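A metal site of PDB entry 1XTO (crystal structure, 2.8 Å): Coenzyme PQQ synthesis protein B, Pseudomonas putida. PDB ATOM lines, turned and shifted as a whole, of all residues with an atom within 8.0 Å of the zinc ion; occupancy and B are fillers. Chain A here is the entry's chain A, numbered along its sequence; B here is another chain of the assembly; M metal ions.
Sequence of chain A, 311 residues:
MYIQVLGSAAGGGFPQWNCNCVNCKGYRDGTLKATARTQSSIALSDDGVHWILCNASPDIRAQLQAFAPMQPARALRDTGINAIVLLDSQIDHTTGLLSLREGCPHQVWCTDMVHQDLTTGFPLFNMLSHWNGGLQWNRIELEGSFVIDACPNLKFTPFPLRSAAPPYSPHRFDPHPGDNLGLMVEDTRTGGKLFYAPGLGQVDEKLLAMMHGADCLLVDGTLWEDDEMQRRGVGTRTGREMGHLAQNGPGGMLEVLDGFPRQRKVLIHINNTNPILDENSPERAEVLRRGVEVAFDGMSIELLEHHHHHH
Asn 272 touches the zinc ion (OD1 to ZN, 2.9 Å). Four residues have an atom within 4 Å of the zinc ion: Cys 19, Cys 21, Cys 24 and Asn 272. The nearest printed residue that does not touch the zinc ion is Gln 16 (4.6 Å).
The zinc ion is bound by the side-chain sulfur of Cys 24 (2.4 Å), the side-chain sulfur of Cys 21 (2.5 Å) and the side-chain sulfur of Cys 19 (2.5 Å).
The backbone NH (N) of Gln 16 lies close to the side-chain sulfur (SG) of Cys 24 (3.5 Å). SG of Cys 21 sits close to N of Asn 23. The backbone carbonyl oxygen (O) of Cys 19 is in hydrogen-bond range of the guanidinium group (NH1) of Arg 28 (2.6 Å). ND2 of Asn 272 lies close to NE2 of Gln 16, at 3.5 Å. ND2 of Asn 23 lies within hydrogen-bond range of O of Asn 272. OD1 of Asn 271 lies within hydrogen-bond range of ND2 of Asn 272 (3.5 Å). O of Gly 13 sits at hydrogen-bond distance from ND2 of Asn 272, at 3.2 Å.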
ATOM      1  N   GLY A  12     -11.680 -28.502  21.859  1.00  0.00           N
ATOM      2  CA  GLY A  12     -11.549 -27.560  22.964  1.00  0.00           C
ATOM      3  C   GLY A  12     -12.192 -26.226  22.661  1.00  0.00           C
ATOM      4  O   GLY A  12     -11.866 -25.207  23.282  1.00  0.00           O
ATOM      5  N   GLY A  13     -13.113 -26.228  21.703  1.00  0.00           N
ATOM      6  CA  GLY A  13     -13.795 -25.009  21.308  1.00  0.00           C
ATOM      7  C   GLY A  13     -12.849 -23.952  20.781  1.00  0.00           C
ATOM      8  O   GLY A  13     -11.828 -24.278  20.183  1.00  0.00           O
ATOM      9  N   PHE A  14     -13.193 -22.694  20.976  1.00  0.00           N
ATOM     10  CA  PHE A  14     -12.335 -21.600  20.512  1.00  0.00           C
ATOM     11  C   PHE A  14     -12.545 -20.304  21.287  1.00  0.00           C
ATOM     12  O   PHE A  14     -13.649 -19.772  21.357  1.00  0.00           O
ATOM     13  CB  PHE A  14     -12.535 -21.355  19.008  1.00  0.00           C
ATOM     14  CG  PHE A  14     -11.772 -20.157  18.478  1.00  0.00           C
ATOM     15  CD1 PHE A  14     -10.380 -20.118  18.539  1.00  0.00           C
ATOM     16  CD2 PHE A  14     -12.458 -19.044  17.992  1.00  0.00           C
ATOM     17  CE1 PHE A  14      -9.678 -18.985  18.129  1.00  0.00           C
ATOM     18  CE2 PHE A  14     -11.764 -17.906  17.572  1.00  0.00           C
ATOM     19  CZ  PHE A  14     -10.377 -17.872  17.646  1.00  0.00           C
ATOM     20  N   PRO A  15     -11.469 -19.786  21.904  1.00  0.00           N
ATOM     21  CA  PRO A  15     -10.121 -20.349  21.895  1.00  0.00           C
ATOM     22  C   PRO A  15     -10.004 -21.545  22.871  1.00  0.00           C
ATOM     23  O   PRO A  15     -10.737 -21.614  23.860  1.00  0.00           O
ATOM     24  CB  PRO A  15      -9.262 -19.169  22.309  1.00  0.00           C
ATOM     25  CG  PRO A  15     -10.147 -18.464  23.309  1.00  0.00           C
ATOM     26  CD  PRO A  15     -11.506 -18.510  22.637  1.00  0.00           C
ATOM     27  N   GLN A  16      -9.088 -22.468  22.601  1.00  0.00           N
ATOM     28  CA  GLN A  16      -8.914 -23.631  23.474  1.00  0.00           C
ATOM     29  C   GLN A  16      -8.299 -23.256  24.821  1.00  0.00           C
ATOM     30  O   GLN A  16      -7.364 -22.462  24.886  1.00  0.00           O
ATOM     31  CB  GLN A  16      -8.036 -24.682  22.801  1.00  0.00           C
ATOM     32  CG  GLN A  16      -8.799 -25.950  22.532  1.00  0.00           C
ATOM     33  CD  GLN A  16      -7.926 -27.170  22.554  1.00  0.00           C
ATOM     34  OE1 GLN A  16      -7.157 -27.390  23.498  1.00  0.00           O
ATOM     35  NE2 GLN A  16      -8.056 -28.008  21.531  1.00  0.00           N
ATOM     36  N   TRP A  17      -8.827 -23.824  25.897  1.00  0.00           N
ATOM     37  CA  TRP A  17      -8.337 -23.509  27.231  1.00  0.00           C
ATOM     38  C   TRP A  17      -6.817 -23.495  27.386  1.00  0.00           C
ATOM     39  O   TRP A  17      -6.263 -22.626  28.055  1.00  0.00           O
ATOM     40  CB  TRP A  17      -8.933 -24.458  28.268  1.00  0.00           C
ATOM     41  CG  TRP A  17      -8.353 -25.843  28.230  1.00  0.00           C
ATOM     42  CD1 TRP A  17      -8.578 -26.813  27.296  1.00  0.00           C
ATOM     43  CD2 TRP A  17      -7.430 -26.396  29.162  1.00  0.00           C
ATOM     44  NE1 TRP A  17      -7.860 -27.935  27.589  1.00  0.00           N
ATOM     45  CE2 TRP A  17      -7.143 -27.712  28.730  1.00  0.00           C
ATOM     46  CE3 TRP A  17      -6.811 -25.914  30.329  1.00  0.00           C
ATOM     47  CZ2 TRP A  17      -6.264 -28.561  29.432  1.00  0.00           C
ATOM     48  CZ3 TRP A  17      -5.933 -26.748  31.028  1.00  0.00           C
ATOM     49  CH2 TRP A  17      -5.672 -28.064  30.570  1.00  0.00           C
ATOM     50  N   ASN A  18      -6.137 -24.464  26.778  1.00  0.00           N
ATOM     51  CA  ASN A  18      -4.684 -24.565  26.919  1.00  0.00           C
ATOM     52  C   ASN A  18      -3.841 -24.319  25.671  1.00  0.00           C
ATOM     53  O   ASN A  18      -2.647 -24.608  25.666  1.00  0.00           O
ATOM     54  CB  ASN A  18      -4.322 -25.937  27.497  1.00  0.00           C
ATOM     55  CG  ASN A  18      -4.555 -27.076  26.517  1.00  0.00           C
ATOM     56  OD1 ASN A  18      -3.895 -28.113  26.606  1.00  0.00           O
ATOM     57  ND2 ASN A  18      -5.499 -26.911  25.600  1.00  0.00           N
ATOM     58  N   CYS A  19      -4.454 -23.756  24.631  1.00  0.00           N
ATOM     59  CA  CYS A  19      -3.772 -23.506  23.373  1.00  0.00           C
ATOM     60  C   CYS A  19      -3.387 -22.053  23.127  1.00  0.00           C
ATOM     61  O   CYS A  19      -4.229 -21.154  23.157  1.00  0.00           O
ATOM     62  CB  CYS A  19      -4.635 -24.000  22.217  1.00  0.00           C
ATOM     63  SG  CYS A  19      -3.768 -24.078  20.648  1.00  0.00           S
ATOM     64  N   ASN A  20      -2.102 -21.835  22.858  1.00  0.00           N
ATOM     65  CA  ASN A  20      -1.618 -20.482  22.591  1.00  0.00           C
ATOM     66  C   ASN A  20      -1.148 -20.312  21.144  1.00  0.00           C
ATOM     67  O   ASN A  20      -0.147 -19.651  20.890  1.00  0.00           O
ATOM     68  CB  ASN A  20      -0.476 -20.142  23.557  1.00  0.00           C
ATOM     69  CG  ASN A  20      -0.926 -20.145  25.006  1.00  0.00           C
ATOM     70  OD1 ASN A  20      -1.725 -19.303  25.416  1.00  0.00           O
ATOM     71  ND2 ASN A  20      -0.406 -21.099  25.784  1.00  0.00           N
ATOM     72  N   CYS A  21      -1.883 -20.905  20.212  1.00  0.00           N
ATOM     73  CA  CYS A  21      -1.527 -20.812  18.804  1.00  0.00           C
ATOM     74  C   CYS A  21      -1.865 -19.430  18.231  1.00  0.00           C
ATOM     75  O   CYS A  21      -2.280 -18.529  18.966  1.00  0.00           O
ATOM     76  CB  CYS A  21      -2.232 -21.901  17.984  1.00  0.00           C
ATOM     77  SG  CYS A  21      -4.005 -21.629  17.777  1.00  0.00           S
ATOM     78  N   VAL A  22      -1.707 -19.286  16.915  1.00  0.00           N
ATOM     79  CA  VAL A  22      -1.988 -18.032  16.232  1.00  0.00           C
ATOM     80  C   VAL A  22      -3.412 -17.521  16.465  1.00  0.00           C
ATOM     81  O   VAL A  22      -3.604 -16.395  16.929  1.00  0.00           O
ATOM     82  CB  VAL A  22      -1.734 -18.166  14.696  1.00  0.00           C
ATOM     83  CG1 VAL A  22      -2.440 -19.388  14.145  1.00  0.00           C
ATOM     84  CG2 VAL A  22      -2.226 -16.904  13.971  1.00  0.00           C
ATOM     85  N   ASN A  23      -4.404 -18.347  16.159  1.00  0.00           N
ATOM     86  CA  ASN A  23      -5.796 -17.962  16.330  1.00  0.00           C
ATOM     87  C   ASN A  23      -6.220 -17.746  17.779  1.00  0.00           C
ATOM     88  O   ASN A  23      -7.023 -16.848  18.072  1.00  0.00           O
ATOM     89  CB  ASN A  23      -6.708 -19.009  15.699  1.00  0.00           C
ATOM     90  CG  ASN A  23      -6.586 -19.035  14.198  1.00  0.00           C
ATOM     91  OD1 ASN A  23      -5.903 -18.170  13.611  1.00  0.00           O
ATOM     92  ND2 ASN A  23      -7.234 -20.003  13.560  1.00  0.00           N
ATOM     93  N   CYS A  24      -5.682 -18.550  18.687  1.00  0.00           N
ATOM     94  CA  CYS A  24      -6.003 -18.429  20.104  1.00  0.00           C
ATOM     95  C   CYS A  24      -5.175 -17.340  20.784  1.00  0.00           C
ATOM     96  O   CYS A  24      -5.727 -16.440  21.412  1.00  0.00           O
ATOM     97  CB  CYS A  24      -5.798 -19.778  20.802  1.00  0.00           C
ATOM     98  SG  CYS A  24      -6.932 -21.062  20.237  1.00  0.00           S
ATOM     99  N   LYS A  25      -3.848 -17.415  20.664  1.00  0.00           N
ATOM    100  CA  LYS A  25      -3.005 -16.398  21.273  1.00  0.00           C
ATOM    101  C   LYS A  25      -3.370 -15.059  20.673  1.00  0.00           C
ATOM    102  O   LYS A  25      -3.210 -14.011  21.300  1.00  0.00           O
ATOM    103  CB  LYS A  25      -1.530 -16.664  20.987  1.00  0.00           C
ATOM    104  CG  LYS A  25      -0.617 -15.499  21.351  1.00  0.00           C
ATOM    105  CD  LYS A  25       0.833 -15.807  20.974  1.00  0.00           C
ATOM    106  CE  LYS A  25       1.727 -14.587  21.112  1.00  0.00           C
ATOM    107  NZ  LYS A  25       1.312 -13.491  20.188  1.00  0.00           N
ATOM    108  N   GLY A  26      -3.878 -15.115  19.443  1.00  0.00           N
ATOM    109  CA  GLY A  26      -4.279 -13.916  18.734  1.00  0.00           C
ATOM    110  C   GLY A  26      -5.572 -13.353  19.253  1.00  0.00           C
ATOM    111  O   GLY A  26      -5.631 -12.188  19.629  1.00  0.00           O
ATOM    112  N   ARG A  28      -7.046 -13.738  22.007  1.00  0.00           N
ATOM    113  CA  ARG A  28      -6.933 -13.197  23.348  1.00  0.00           C
ATOM    114  C   ARG A  28      -6.192 -11.863  23.346  1.00  0.00           C
ATOM    115  O   ARG A  28      -6.458 -10.992  24.172  1.00  0.00           O
ATOM    116  CB  ARG A  28      -6.250 -14.211  24.283  1.00  0.00           C
ATOM    117  CG  ARG A  28      -7.175 -15.363  24.732  1.00  0.00           C
ATOM    118  CD  ARG A  28      -6.533 -16.232  25.821  1.00  0.00           C
ATOM    119  NE  ARG A  28      -5.802 -17.381  25.273  1.00  0.00           N
ATOM    120  CZ  ARG A  28      -6.227 -18.641  25.340  1.00  0.00           C
ATOM    121  NH1 ARG A  28      -5.496 -19.600  24.803  1.00  0.00           N
ATOM    122  NH2 ARG A  28      -7.368 -18.940  25.951  1.00  0.00           N
ATOM    123  N   ARG A 232       0.714 -25.528  12.895  1.00  0.00           N
ATOM    124  CA  ARG A 232       0.548 -24.817  14.152  1.00  0.00           C
ATOM    125  C   ARG A 232       1.410 -25.391  15.279  1.00  0.00           C
ATOM    126  O   ARG A 232       1.723 -24.679  16.240  1.00  0.00           O
ATOM    127  CB  ARG A 232      -0.918 -24.833  14.571  1.00  0.00           C
ATOM    128  CG  ARG A 232      -1.868 -24.381  13.468  1.00  0.00           C
ATOM    129  CD  ARG A 232      -1.522 -22.985  12.960  1.00  0.00           C
ATOM    130  NE  ARG A 232      -2.575 -22.455  12.091  1.00  0.00           N
ATOM    131  CZ  ARG A 232      -2.529 -21.276  11.482  1.00  0.00           C
ATOM    132  NH1 ARG A 232      -3.531 -20.881  10.715  1.00  0.00           N
ATOM    133  NH2 ARG A 232      -1.468 -20.493  11.628  1.00  0.00           N
ATOM    134  N   VAL A 234       0.676 -27.896  17.505  1.00  0.00           N
ATOM    135  CA  VAL A 234      -0.047 -28.146  18.740  1.00  0.00           C
ATOM    136  C   VAL A 234      -0.581 -29.582  18.826  1.00  0.00           C
ATOM    137  O   VAL A 234      -0.915 -30.058  19.905  1.00  0.00           O
ATOM    138  CB  VAL A 234      -1.241 -27.183  18.891  1.00  0.00           C
ATOM    139  CG1 VAL A 234      -0.750 -25.750  19.013  1.00  0.00           C
ATOM    140  CG2 VAL A 234      -2.174 -27.328  17.695  1.00  0.00           C
ATOM    141  N   ASN A 271     -12.070 -26.127  14.007  1.00  0.00           N
ATOM    142  CA  ASN A 271     -11.025 -26.287  15.027  1.00  0.00           C
ATOM    143  C   ASN A 271     -10.364 -24.952  15.229  1.00  0.00           C
ATOM    144  O   ASN A 271     -10.367 -24.117  14.329  1.00  0.00           O
ATOM    145  CB  ASN A 271      -9.958 -27.297  14.609  1.00  0.00           C
ATOM    146  CG  ASN A 271      -8.998 -27.665  15.765  1.00  0.00           C
ATOM    147  OD1 ASN A 271      -9.407 -28.267  16.751  1.00  0.00           O
ATOM    148  ND2 ASN A 271      -7.725 -27.299  15.623  1.00  0.00           N
ATOM    149  N   ASN A 272      -9.776 -24.765  16.404  1.00  0.00           N
ATOM    150  CA  ASN A 272      -9.101 -23.518  16.737  1.00  0.00           C
ATOM    151  C   ASN A 272      -7.913 -23.211  15.832  1.00  0.00           C
ATOM    152  O   ASN A 272      -7.521 -22.059  15.670  1.00  0.00           O
ATOM    153  CB  ASN A 272      -8.663 -23.552  18.219  1.00  0.00           C
ATOM    154  CG  ASN A 272      -8.231 -24.951  18.683  1.00  0.00           C
ATOM    155  OD1 ASN A 272      -7.055 -25.303  18.623  1.00  0.00           O
ATOM    156  ND2 ASN A 272      -9.196 -25.749  19.137  1.00  0.00           N
ATOM    157  N   THR A 273      -7.367 -24.250  15.204  1.00  0.00           N
ATOM    158  CA  THR A 273      -6.230 -24.056  14.324  1.00  0.00           C
ATOM    159  C   THR A 273      -6.626 -23.568  12.932  1.00  0.00           C
ATOM    160  O   THR A 273      -5.861 -22.865  12.279  1.00  0.00           O
ATOM    161  CB  THR A 273      -5.433 -25.356  14.222  1.00  0.00           C
ATOM    162  OG1 THR A 273      -6.309 -26.423  13.871  1.00  0.00           O
ATOM    163  CG2 THR A 273      -4.772 -25.664  15.541  1.00  0.00           C
ATOM    164  N   ASN A 274      -7.827 -23.928  12.484  1.00  0.00           N
ATOM    165  CA  ASN A 274      -8.302 -23.539  11.162  1.00  0.00           C
ATOM    166  C   ASN A 274      -8.170 -22.035  10.914  1.00  0.00           C
ATOM    167  O   ASN A 274      -8.668 -21.223  11.696  1.00  0.00           O
ATOM    168  CB  ASN A 274      -9.760 -23.985  10.963  1.00  0.00           C
ATOM    169  CG  ASN A 274     -10.133 -24.131   9.505  1.00  0.00           C
ATOM    170  OD1 ASN A 274      -9.794 -23.282   8.689  1.00  0.00           O
ATOM    171  ND2 ASN A 274     -10.848 -25.202   9.163  1.00  0.00           N
ATOM    172  N   LEU A 277     -10.879 -18.988  10.676  1.00  0.00           N
ATOM    173  CA  LEU A 277     -11.415 -18.393  11.888  1.00  0.00           C
ATOM    174  C   LEU A 277     -10.972 -16.939  11.952  1.00  0.00           C
ATOM    175  O   LEU A 277     -11.376 -16.188  12.833  1.00  0.00           O
ATOM    176  CB  LEU A 277     -10.920 -19.170  13.113  1.00  0.00           C
ATOM    177  CG  LEU A 277     -11.968 -19.694  14.119  1.00  0.00           C
ATOM    178  CD1 LEU A 277     -13.043 -20.476  13.381  1.00  0.00           C
ATOM    179  CD2 LEU A 277     -11.297 -20.576  15.174  1.00  0.00           C
ATOM    180  N   LEU B  76       3.467 -22.617  23.576  1.00  0.00           N
ATOM    181  CA  LEU B  76       2.293 -23.153  22.899  1.00  0.00           C
ATOM    182  C   LEU B  76       1.792 -24.291  23.759  1.00  0.00           C
ATOM    183  O   LEU B  76       2.590 -24.992  24.394  1.00  0.00           O
ATOM    184  CB  LEU B  76       2.649 -23.676  21.520  1.00  0.00           C
ATOM    185  CG  LEU B  76       3.067 -22.639  20.469  1.00  0.00           C
ATOM    186  CD1 LEU B  76       3.243 -23.370  19.151  1.00  0.00           C
ATOM    187  CD2 LEU B  76       2.032 -21.536  20.349  1.00  0.00           C
ATOM    188  N   ARG B  77       0.482 -24.506  23.803  1.00  0.00           N
ATOM    189  CA  ARG B  77      -0.069 -25.582  24.628  1.00  0.00           C
ATOM    190  C   ARG B  77       0.533 -25.484  26.038  1.00  0.00           C
ATOM    191  O   ARG B  77       1.480 -26.186  26.382  1.00  0.00           O
ATOM    192  CB  ARG B  77       0.258 -26.943  24.000  1.00  0.00           C
ATOM    193  CG  ARG B  77      -0.459 -28.121  24.651  1.00  0.00           C
ATOM    194  CD  ARG B  77      -0.615 -29.310  23.688  1.00  0.00           C
ATOM    195  NE  ARG B  77      -1.427 -28.975  22.509  1.00  0.00           N
ATOM    196  CZ  ARG B  77      -2.754 -28.856  22.495  1.00  0.00           C
ATOM    197  NH1 ARG B  77      -3.460 -29.058  23.602  1.00  0.00           N
ATOM    198  NH2 ARG B  77      -3.396 -28.543  21.369  1.00  0.00           N
HETATM  199 ZN    ZN M   1      -5.585 -22.855  19.347  1.00  0.00          ZN
